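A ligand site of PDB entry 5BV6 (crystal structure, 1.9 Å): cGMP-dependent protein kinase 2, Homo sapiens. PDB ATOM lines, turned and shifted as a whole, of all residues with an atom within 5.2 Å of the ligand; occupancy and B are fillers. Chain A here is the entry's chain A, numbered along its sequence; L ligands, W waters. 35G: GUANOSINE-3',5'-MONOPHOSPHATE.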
ATOM      1  N   ILE A  48     -29.122  29.491 -30.522  1.00  0.00           N
ATOM      2  CA  ILE A  48     -29.491  28.095 -30.690  1.00  0.00           C
ATOM      3  C   ILE A  48     -30.646  27.804 -29.740  1.00  0.00           C
ATOM      4  O   ILE A  48     -30.624  28.248 -28.587  1.00  0.00           O
ATOM      5  CB  ILE A  48     -28.317  27.136 -30.359  1.00  0.00           C
ATOM      6  CG1 ILE A  48     -27.304  27.091 -31.504  1.00  0.00           C
ATOM      7  CG2 ILE A  48     -28.837  25.741 -30.064  1.00  0.00           C
ATOM      8  CD1 ILE A  48     -26.046  26.283 -31.167  1.00  0.00           C
ATOM      9  N   VAL A  67     -25.737  29.587 -21.514  1.00  0.00           N
ATOM     10  CA  VAL A  67     -26.196  28.269 -21.900  1.00  0.00           C
ATOM     11  C   VAL A  67     -27.293  27.871 -20.920  1.00  0.00           C
ATOM     12  O   VAL A  67     -27.067  27.881 -19.715  1.00  0.00           O
ATOM     13  CB  VAL A  67     -25.048  27.240 -21.867  1.00  0.00           C
ATOM     14  CG1 VAL A  67     -25.534  25.858 -22.300  1.00  0.00           C
ATOM     15  CG2 VAL A  67     -23.889  27.725 -22.723  1.00  0.00           C
ATOM     16  N   GLN A  69     -30.584  24.925 -20.164  1.00  0.00           N
ATOM     17  CA  GLN A  69     -30.972  23.566 -20.504  1.00  0.00           C
ATOM     18  C   GLN A  69     -32.102  23.045 -19.621  1.00  0.00           C
ATOM     19  O   GLN A  69     -32.125  23.277 -18.411  1.00  0.00           O
ATOM     20  CB  GLN A  69     -29.757  22.647 -20.399  1.00  0.00           C
ATOM     21  CG  GLN A  69     -30.006  21.231 -20.864  1.00  0.00           C
ATOM     22  CD  GLN A  69     -28.767  20.388 -20.754  1.00  0.00           C
ATOM     23  OE1 GLN A  69     -28.319  20.090 -19.648  1.00  0.00           O
ATOM     24  NE2 GLN A  69     -28.191  20.005 -21.891  1.00  0.00           N
ATOM     25  N   ILE A  80     -26.715  27.006 -16.954  1.00  0.00           N
ATOM     26  CA  ILE A  80     -25.586  26.088 -16.751  1.00  0.00           C
ATOM     27  C   ILE A  80     -24.248  26.814 -16.702  1.00  0.00           C
ATOM     28  O   ILE A  80     -23.356  26.507 -15.903  1.00  0.00           O
ATOM     29  CB  ILE A  80     -25.524  25.006 -17.878  1.00  0.00           C
ATOM     30  CG1 ILE A  80     -26.444  23.828 -17.552  1.00  0.00           C
ATOM     31  CG2 ILE A  80     -24.108  24.447 -18.033  1.00  0.00           C
ATOM     32  CD1 ILE A  80     -27.899  24.122 -17.619  1.00  0.00           C
ATOM     33  N   LYS A  81     -24.092  27.783 -17.595  1.00  0.00           N
ATOM     34  CA  LYS A  81     -22.829  28.523 -17.689  1.00  0.00           C
ATOM     35  C   LYS A  81     -22.940  29.678 -18.688  1.00  0.00           C
ATOM     36  O   LYS A  81     -23.906  29.766 -19.430  1.00  0.00           O
ATOM     37  CB  LYS A  81     -21.676  27.603 -18.120  1.00  0.00           C
ATOM     38  CG  LYS A  81     -21.756  27.178 -19.583  1.00  0.00           C
ATOM     39  CD  LYS A  81     -20.615  26.267 -19.989  1.00  0.00           C
ATOM     40  CE  LYS A  81     -20.848  24.843 -19.531  1.00  0.00           C
ATOM     41  NZ  LYS A  81     -19.976  23.889 -20.284  1.00  0.00           N
ATOM     42  N   LEU A  83     -20.569  31.600 -21.818  1.00  0.00           N
ATOM     43  CA  LEU A  83     -19.392  31.513 -22.666  1.00  0.00           C
ATOM     44  C   LEU A  83     -18.981  32.885 -23.164  1.00  0.00           C
ATOM     45  O   LEU A  83     -19.822  33.766 -23.340  1.00  0.00           O
ATOM     46  CB  LEU A  83     -19.646  30.592 -23.855  1.00  0.00           C
ATOM     47  CG  LEU A  83     -20.043  29.150 -23.534  1.00  0.00           C
ATOM     48  CD1 LEU A  83     -20.432  28.436 -24.812  1.00  0.00           C
ATOM     49  CD2 LEU A  83     -18.883  28.442 -22.861  1.00  0.00           C
ATOM     50  N   TYR A  88     -16.548  28.412 -28.001  1.00  0.00           N
ATOM     51  CA  TYR A  88     -17.339  27.908 -29.120  1.00  0.00           C
ATOM     52  C   TYR A  88     -18.492  27.044 -28.632  1.00  0.00           C
ATOM     53  O   TYR A  88     -18.521  26.612 -27.473  1.00  0.00           O
ATOM     54  CB  TYR A  88     -16.450  27.114 -30.073  1.00  0.00           C
ATOM     55  CG  TYR A  88     -15.646  26.009 -29.394  1.00  0.00           C
ATOM     56  CD1 TYR A  88     -16.209  24.766 -29.161  1.00  0.00           C
ATOM     57  CD2 TYR A  88     -14.336  26.212 -28.995  1.00  0.00           C
ATOM     58  CE1 TYR A  88     -15.493  23.757 -28.544  1.00  0.00           C
ATOM     59  CE2 TYR A  88     -13.597  25.212 -28.394  1.00  0.00           C
ATOM     60  CZ  TYR A  88     -14.188  23.991 -28.171  1.00  0.00           C
ATOM     61  OH  TYR A  88     -13.461  22.991 -27.563  1.00  0.00           O
ATOM     62  N   PHE A  89     -19.433  26.776 -29.534  1.00  0.00           N
ATOM     63  CA  PHE A  89     -20.571  25.934 -29.197  1.00  0.00           C
ATOM     64  C   PHE A  89     -21.224  25.411 -30.455  1.00  0.00           C
ATOM     65  O   PHE A  89     -20.954  25.898 -31.560  1.00  0.00           O
ATOM     66  CB  PHE A  89     -21.593  26.713 -28.345  1.00  0.00           C
ATOM     67  CG  PHE A  89     -22.044  28.015 -28.972  1.00  0.00           C
ATOM     68  CD1 PHE A  89     -23.105  28.031 -29.858  1.00  0.00           C
ATOM     69  CD2 PHE A  89     -21.429  29.210 -28.644  1.00  0.00           C
ATOM     70  CE1 PHE A  89     -23.542  29.242 -30.446  1.00  0.00           C
ATOM     71  CE2 PHE A  89     -21.843  30.435 -29.215  1.00  0.00           C
ATOM     72  CZ  PHE A  89     -22.909  30.444 -30.112  1.00  0.00           C
ATOM     73  N   GLY A  90     -22.072  24.400 -30.296  1.00  0.00           N
ATOM     74  CA  GLY A  90     -22.795  23.857 -31.439  1.00  0.00           C
ATOM     75  C   GLY A  90     -22.177  22.614 -32.039  1.00  0.00           C
ATOM     76  O   GLY A  90     -22.756  22.007 -32.945  1.00  0.00           O
ATOM     77  N   GLU A  91     -20.996  22.236 -31.546  1.00  0.00           N
ATOM     78  CA  GLU A  91     -20.310  21.064 -32.060  1.00  0.00           C
ATOM     79  C   GLU A  91     -21.073  19.796 -31.724  1.00  0.00           C
ATOM     80  O   GLU A  91     -21.023  18.815 -32.466  1.00  0.00           O
ATOM     81  CB  GLU A  91     -18.867  20.972 -31.518  1.00  0.00           C
ATOM     82  CG  GLU A  91     -18.771  20.601 -30.037  1.00  0.00           C
ATOM     83  CD  GLU A  91     -19.438  21.646 -29.157  1.00  0.00           C
ATOM     84  OE1 GLU A  91     -19.136  22.840 -29.350  1.00  0.00           O
ATOM     85  OE2 GLU A  91     -20.289  21.293 -28.313  1.00  0.00           O
ATOM     86  N   LYS A  92     -21.793  19.801 -30.606  1.00  0.00           N
ATOM     87  CA  LYS A  92     -22.396  18.553 -30.125  1.00  0.00           C
ATOM     88  C   LYS A  92     -23.424  17.975 -31.104  1.00  0.00           C
ATOM     89  O   LYS A  92     -23.474  16.759 -31.309  1.00  0.00           O
ATOM     90  CB  LYS A  92     -23.053  18.741 -28.756  1.00  0.00           C
ATOM     91  CG  LYS A  92     -23.335  17.418 -28.011  1.00  0.00           C
ATOM     92  CD  LYS A  92     -24.066  17.664 -26.697  1.00  0.00           C
ATOM     93  CE  LYS A  92     -24.055  16.420 -25.803  1.00  0.00           C
ATOM     94  NZ  LYS A  92     -24.676  15.256 -26.491  1.00  0.00           N
ATOM     95  N   ALA A  93     -24.259  18.825 -31.705  1.00  0.00           N
ATOM     96  CA  ALA A  93     -25.264  18.289 -32.631  1.00  0.00           C
ATOM     97  C   ALA A  93     -24.615  17.603 -33.823  1.00  0.00           C
ATOM     98  O   ALA A  93     -25.149  16.637 -34.359  1.00  0.00           O
ATOM     99  CB  ALA A  93     -26.211  19.406 -33.113  1.00  0.00           C
ATOM    100  N   LEU A  94     -23.473  18.110 -34.244  1.00  0.00           N
ATOM    101  CA  LEU A  94     -22.788  17.568 -35.415  1.00  0.00           C
ATOM    102  C   LEU A  94     -22.077  16.260 -35.084  1.00  0.00           C
ATOM    103  O   LEU A  94     -22.213  15.271 -35.791  1.00  0.00           O
ATOM    104  CB  LEU A  94     -21.803  18.587 -35.965  1.00  0.00           C
ATOM    105  CG  LEU A  94     -22.457  19.801 -36.617  1.00  0.00           C
ATOM    106  CD1 LEU A  94     -21.530  21.012 -36.640  1.00  0.00           C
ATOM    107  CD2 LEU A  94     -22.854  19.429 -38.034  1.00  0.00           C
ATOM    108  N   VAL A  99     -30.272  16.490 -32.182  1.00  0.00           N
ATOM    109  CA  VAL A  99     -30.846  17.825 -32.150  1.00  0.00           C
ATOM    110  C   VAL A  99     -30.051  18.646 -31.133  1.00  0.00           C
ATOM    111  O   VAL A  99     -29.330  18.071 -30.301  1.00  0.00           O
ATOM    112  CB  VAL A  99     -32.344  17.817 -31.780  1.00  0.00           C
ATOM    113  CG1 VAL A  99     -33.131  16.956 -32.767  1.00  0.00           C
ATOM    114  CG2 VAL A  99     -32.537  17.319 -30.359  1.00  0.00           C
ATOM    115  N   ARG A 100     -30.147  19.975 -31.230  1.00  0.00           N
ATOM    116  CA  ARG A 100     -29.502  20.870 -30.261  1.00  0.00           C
ATOM    117  C   ARG A 100     -29.871  20.475 -28.840  1.00  0.00           C
ATOM    118  O   ARG A 100     -31.038  20.206 -28.550  1.00  0.00           O
ATOM    119  CB  ARG A 100     -29.915  22.333 -30.525  1.00  0.00           C
ATOM    120  CG  ARG A 100     -29.562  22.847 -31.903  1.00  0.00           C
ATOM    121  CD  ARG A 100     -28.048  22.890 -32.117  1.00  0.00           C
ATOM    122  NE  ARG A 100     -27.696  23.696 -33.290  1.00  0.00           N
ATOM    123  CZ  ARG A 100     -26.488  23.699 -33.846  1.00  0.00           C
ATOM    124  NH1 ARG A 100     -25.527  22.941 -33.336  1.00  0.00           N
ATOM    125  NH2 ARG A 100     -26.237  24.476 -34.904  1.00  0.00           N
ATOM    126  N   SER A 101     -28.886  20.476 -27.948  1.00  0.00           N
ATOM    127  CA  SER A 101     -29.063  19.894 -26.617  1.00  0.00           C
ATOM    128  C   SER A 101     -29.165  20.955 -25.512  1.00  0.00           C
ATOM    129  O   SER A 101     -29.338  20.643 -24.333  1.00  0.00           O
ATOM    130  CB  SER A 101     -27.903  18.940 -26.317  1.00  0.00           C
ATOM    131  OG  SER A 101     -26.671  19.665 -26.212  1.00  0.00           O
ATOM    132  N   ALA A 102     -29.078  22.223 -25.909  1.00  0.00           N
ATOM    133  CA  ALA A 102     -29.199  23.346 -24.973  1.00  0.00           C
ATOM    134  C   ALA A 102     -29.515  24.632 -25.730  1.00  0.00           C
ATOM    135  O   ALA A 102     -29.319  24.694 -26.946  1.00  0.00           O
ATOM    136  CB  ALA A 102     -27.923  23.520 -24.164  1.00  0.00           C
ATOM    137  N   ILE A 104     -28.632  28.526 -26.502  1.00  0.00           N
ATOM    138  CA  ILE A 104     -27.541  29.484 -26.429  1.00  0.00           C
ATOM    139  C   ILE A 104     -28.108  30.874 -26.643  1.00  0.00           C
ATOM    140  O   ILE A 104     -28.651  31.162 -27.719  1.00  0.00           O
ATOM    141  CB  ILE A 104     -26.464  29.208 -27.473  1.00  0.00           C
ATOM    142  CG1 ILE A 104     -25.951  27.764 -27.343  1.00  0.00           C
ATOM    143  CG2 ILE A 104     -25.333  30.181 -27.295  1.00  0.00           C
ATOM    144  CD1 ILE A 104     -25.134  27.542 -26.112  1.00  0.00           C
ATOM    145  N   TYR A 138     -14.474  16.342 -25.553  1.00  0.00           N
ATOM    146  CA  TYR A 138     -15.244  17.501 -25.117  1.00  0.00           C
ATOM    147  C   TYR A 138     -16.730  17.152 -25.034  1.00  0.00           C
ATOM    148  O   TYR A 138     -17.396  17.414 -24.030  1.00  0.00           O
ATOM    149  CB  TYR A 138     -14.991  18.674 -26.086  1.00  0.00           C
ATOM    150  CG  TYR A 138     -15.696  19.972 -25.752  1.00  0.00           C
ATOM    151  CD1 TYR A 138     -15.116  20.894 -24.903  1.00  0.00           C
ATOM    152  CD2 TYR A 138     -16.913  20.278 -26.328  1.00  0.00           C
ATOM    153  CE1 TYR A 138     -15.753  22.085 -24.616  1.00  0.00           C
ATOM    154  CE2 TYR A 138     -17.561  21.474 -26.047  1.00  0.00           C
ATOM    155  CZ  TYR A 138     -16.983  22.366 -25.188  1.00  0.00           C
ATOM    156  OH  TYR A 138     -17.625  23.550 -24.912  1.00  0.00           O
ATOM    157  N   LEU A 142     -19.498  16.789 -21.977  1.00  0.00           N
ATOM    158  CA  LEU A 142     -20.826  17.410 -21.978  1.00  0.00           C
ATOM    159  C   LEU A 142     -21.879  16.375 -21.590  1.00  0.00           C
ATOM    160  O   LEU A 142     -22.760  16.647 -20.780  1.00  0.00           O
ATOM    161  CB  LEU A 142     -21.160  18.010 -23.349  1.00  0.00           C
ATOM    162  CG  LEU A 142     -20.246  19.120 -23.860  1.00  0.00           C
ATOM    163  CD1 LEU A 142     -20.832  19.756 -25.115  1.00  0.00           C
ATOM    164  CD2 LEU A 142     -20.040  20.158 -22.782  1.00  0.00           C
ATOM    165  N   ASP A 145     -21.863  15.762 -17.957  1.00  0.00           N
ATOM    166  CA  ASP A 145     -22.485  16.911 -17.289  1.00  0.00           C
ATOM    167  C   ASP A 145     -24.007  16.835 -17.379  1.00  0.00           C
ATOM    168  O   ASP A 145     -24.692  17.040 -16.387  1.00  0.00           O
ATOM    169  CB  ASP A 145     -21.991  18.242 -17.896  1.00  0.00           C
ATOM    170  CG  ASP A 145     -20.552  18.541 -17.532  1.00  0.00           C
ATOM    171  OD1 ASP A 145     -20.026  17.880 -16.607  1.00  0.00           O
ATOM    172  OD2 ASP A 145     -19.933  19.440 -18.157  1.00  0.00           O
ATOM    173  N   ASP A 146     -24.530  16.524 -18.574  1.00  0.00           N
ATOM    174  CA  ASP A 146     -25.971  16.396 -18.747  1.00  0.00           C
ATOM    175  C   ASP A 146     -26.499  15.327 -17.789  1.00  0.00           C
ATOM    176  O   ASP A 146     -27.525  15.527 -17.144  1.00  0.00           O
ATOM    177  CB  ASP A 146     -26.343  16.039 -20.193  1.00  0.00           C
ATOM    178  CG  ASP A 146     -26.056  17.168 -21.177  1.00  0.00           C
ATOM    179  OD1 ASP A 146     -25.682  18.278 -20.753  1.00  0.00           O
ATOM    180  OD2 ASP A 146     -26.233  16.937 -22.396  1.00  0.00           O
ATOM    181  N   ARG A 149     -26.721  16.664 -14.021  1.00  0.00           N
ATOM    182  CA  ARG A 149     -27.799  17.587 -13.696  1.00  0.00           C
ATOM    183  C   ARG A 149     -29.185  17.053 -14.101  1.00  0.00           C
ATOM    184  O   ARG A 149     -30.189  17.747 -13.937  1.00  0.00           O
ATOM    185  CB  ARG A 149     -27.561  18.949 -14.382  1.00  0.00           C
ATOM    186  CG  ARG A 149     -27.826  18.941 -15.872  1.00  0.00           C
ATOM    187  CD  ARG A 149     -27.644  20.361 -16.454  1.00  0.00           C
ATOM    188  NE  ARG A 149     -26.252  20.775 -16.349  1.00  0.00           N
ATOM    189  CZ  ARG A 149     -25.376  20.652 -17.344  1.00  0.00           C
ATOM    190  NH1 ARG A 149     -25.751  20.161 -18.522  1.00  0.00           N
ATOM    191  NH2 ARG A 149     -24.119  21.034 -17.160  1.00  0.00           N
HETATM  192  P   35G L   1     -25.358  21.652 -29.413  1.00  0.00           P
HETATM  193  O1P 35G L   1     -25.264  21.520 -30.811  1.00  0.00           O
HETATM  194  O2P 35G L   1     -26.136  20.698 -28.746  1.00  0.00           O
HETATM  195  O5' 35G L   1     -26.072  22.966 -29.112  1.00  0.00           O
HETATM  196  C5' 35G L   1     -26.129  23.502 -27.819  1.00  0.00           C
HETATM  197  C4' 35G L   1     -24.698  23.618 -27.335  1.00  0.00           C
HETATM  198  O4' 35G L   1     -24.466  24.079 -26.048  1.00  0.00           O
HETATM  199  C3' 35G L   1     -23.941  22.315 -27.424  1.00  0.00           C
HETATM  200  O3' 35G L   1     -23.956  21.909 -28.761  1.00  0.00           O
HETATM  201  C2' 35G L   1     -22.643  22.707 -26.719  1.00  0.00           C
HETATM  202  O2' 35G L   1     -21.749  23.354 -27.544  1.00  0.00           O
HETATM  203  C1' 35G L   1     -23.128  23.748 -25.732  1.00  0.00           C
HETATM  204  N9  35G L   1     -23.005  23.327 -24.347  1.00  0.00           N
HETATM  205  C8  35G L   1     -22.373  24.000 -23.407  1.00  0.00           C
HETATM  206  N7  35G L   1     -22.439  23.403 -22.239  1.00  0.00           N
HETATM  207  C5  35G L   1     -23.145  22.323 -22.419  1.00  0.00           C
HETATM  208  C6  35G L   1     -23.602  21.212 -21.564  1.00  0.00           C
HETATM  209  O6  35G L   1     -23.317  21.180 -20.385  1.00  0.00           O
HETATM  210  N1  35G L   1     -24.329  20.260 -22.110  1.00  0.00           N
HETATM  211  C2  35G L   1     -24.644  20.248 -23.390  1.00  0.00           C
HETATM  212  N2  35G L   1     -25.351  19.200 -23.835  1.00  0.00           N
HETATM  213  N3  35G L   1     -24.259  21.247 -24.225  1.00  0.00           N
HETATM  214  C4  35G L   1     -23.517  22.256 -23.808  1.00  0.00           C
HETATM  215  O   HOH W   1     -19.819  24.652 -26.029  1.00  0.00           O
HETATM  216  O   HOH W   2     -26.692  17.938 -29.543  1.00  0.00           O
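The side-chain carboxylate (OE2) of Glu 91 sits at hydrogen-bond distance from an oxygen (O2') of the ligand (2.6 Å). OD1 of Asp 146 is in hydrogen-bond range of N1 of the ligand (2.8 Å). The backbone NH (N) of Ser 101 is in hydrogen-bond range of an oxygen (O2P) of the ligand, at 2.9 Å. The side-chain hydroxyl (OG) of Ser 101 is in hydrogen-bond range of a nitrogen (N2) of the ligand. An oxygen (O1P) of the ligand is in salt-bridge range of the guanidinium group (NH1) of Arg 100 (2.9 Å). O2' of the ligand lies within hydrogen-bond range of N of Gly 90. N of Ala 93 is in hydrogen-bond range of O1P of the ligand (3.0 Å). NZ of Lys 81 lies within hydrogen-bond range of N7 of the ligand, at 3.2 Å. O6 of the ligand lies within hydrogen-bond range of NH1 of Arg 149.
The guanidinium group (NH1) of Arg 149 lies within salt-bridge range of the side-chain carboxylate (OD1) of Asp 146, at 2.9 Å. The side-chain amide nitrogen of Gln 69 lies within hydrogen-bond range of the side-chain carboxylate of Asp 146, at 3.3 Å. The backbone carbonyl oxygen of Ser 101 lies within hydrogen-bond range of the side-chain amide nitrogen of Gln 69. The guanidinium group (NH1) of Arg 100 lies within hydrogen-bond range of the backbone carbonyl oxygen (O) of Gly 90. The backbone carbonyl oxygen (O) of Lys 81 lies within hydrogen-bond range of the backbone NH (N) of Val 67 (2.8 Å). The guanidinium group (NH1) of Arg 149 lies within hydrogen-bond range of the side-chain amide oxygen (OE1) of Gln 69, at 2.8 Å. N of Ile 104 sits at hydrogen-bond distance from O of Ile 48 (2.9 Å). The backbone NH of Ile 80 lies within hydrogen-bond range of the backbone carbonyl oxygen of Val 67 (2.9 Å).
CD1 of Ile 48 touches O5' of the ligand (3.9 Å). CG1 of Val 67 touches C8 of the ligand (3.8 Å). Gln 69 touches the ligand (NE2 to N2, 3.5 Å). Phe 89 touches the ligand (CA to O2', 3.3 Å). Lys 92 touches the ligand. Ala 102 touches the ligand. Ile 104 touches the ligand (CD1 to O4', 3.5 Å). CD2 of Leu 142 touches C5 of the ligand (3.8 Å). Hydrophobic or aromatic side chains within 4 Å of the ligand: Ile 48, Val 67, Phe 89, Ala 93, Ala 102, Ile 104 and Leu 142. The nearest printed residue that does not touch the ligand is Asp 145 (4.1 Å).
Water W1 lies within hydrogen-bond range of the side-chain hydroxyl (OH) of Tyr 138 (2.7 Å), the backbone carbonyl oxygen (O) of Tyr 88 (2.8 Å) and an oxygen (O2') of the ligand (2.8 Å). Water W2 lies within hydrogen-bond range of O of Val 99 (2.7 Å), O2P of the ligand (2.9 Å) and N of Ala 93 (3.4 Å).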
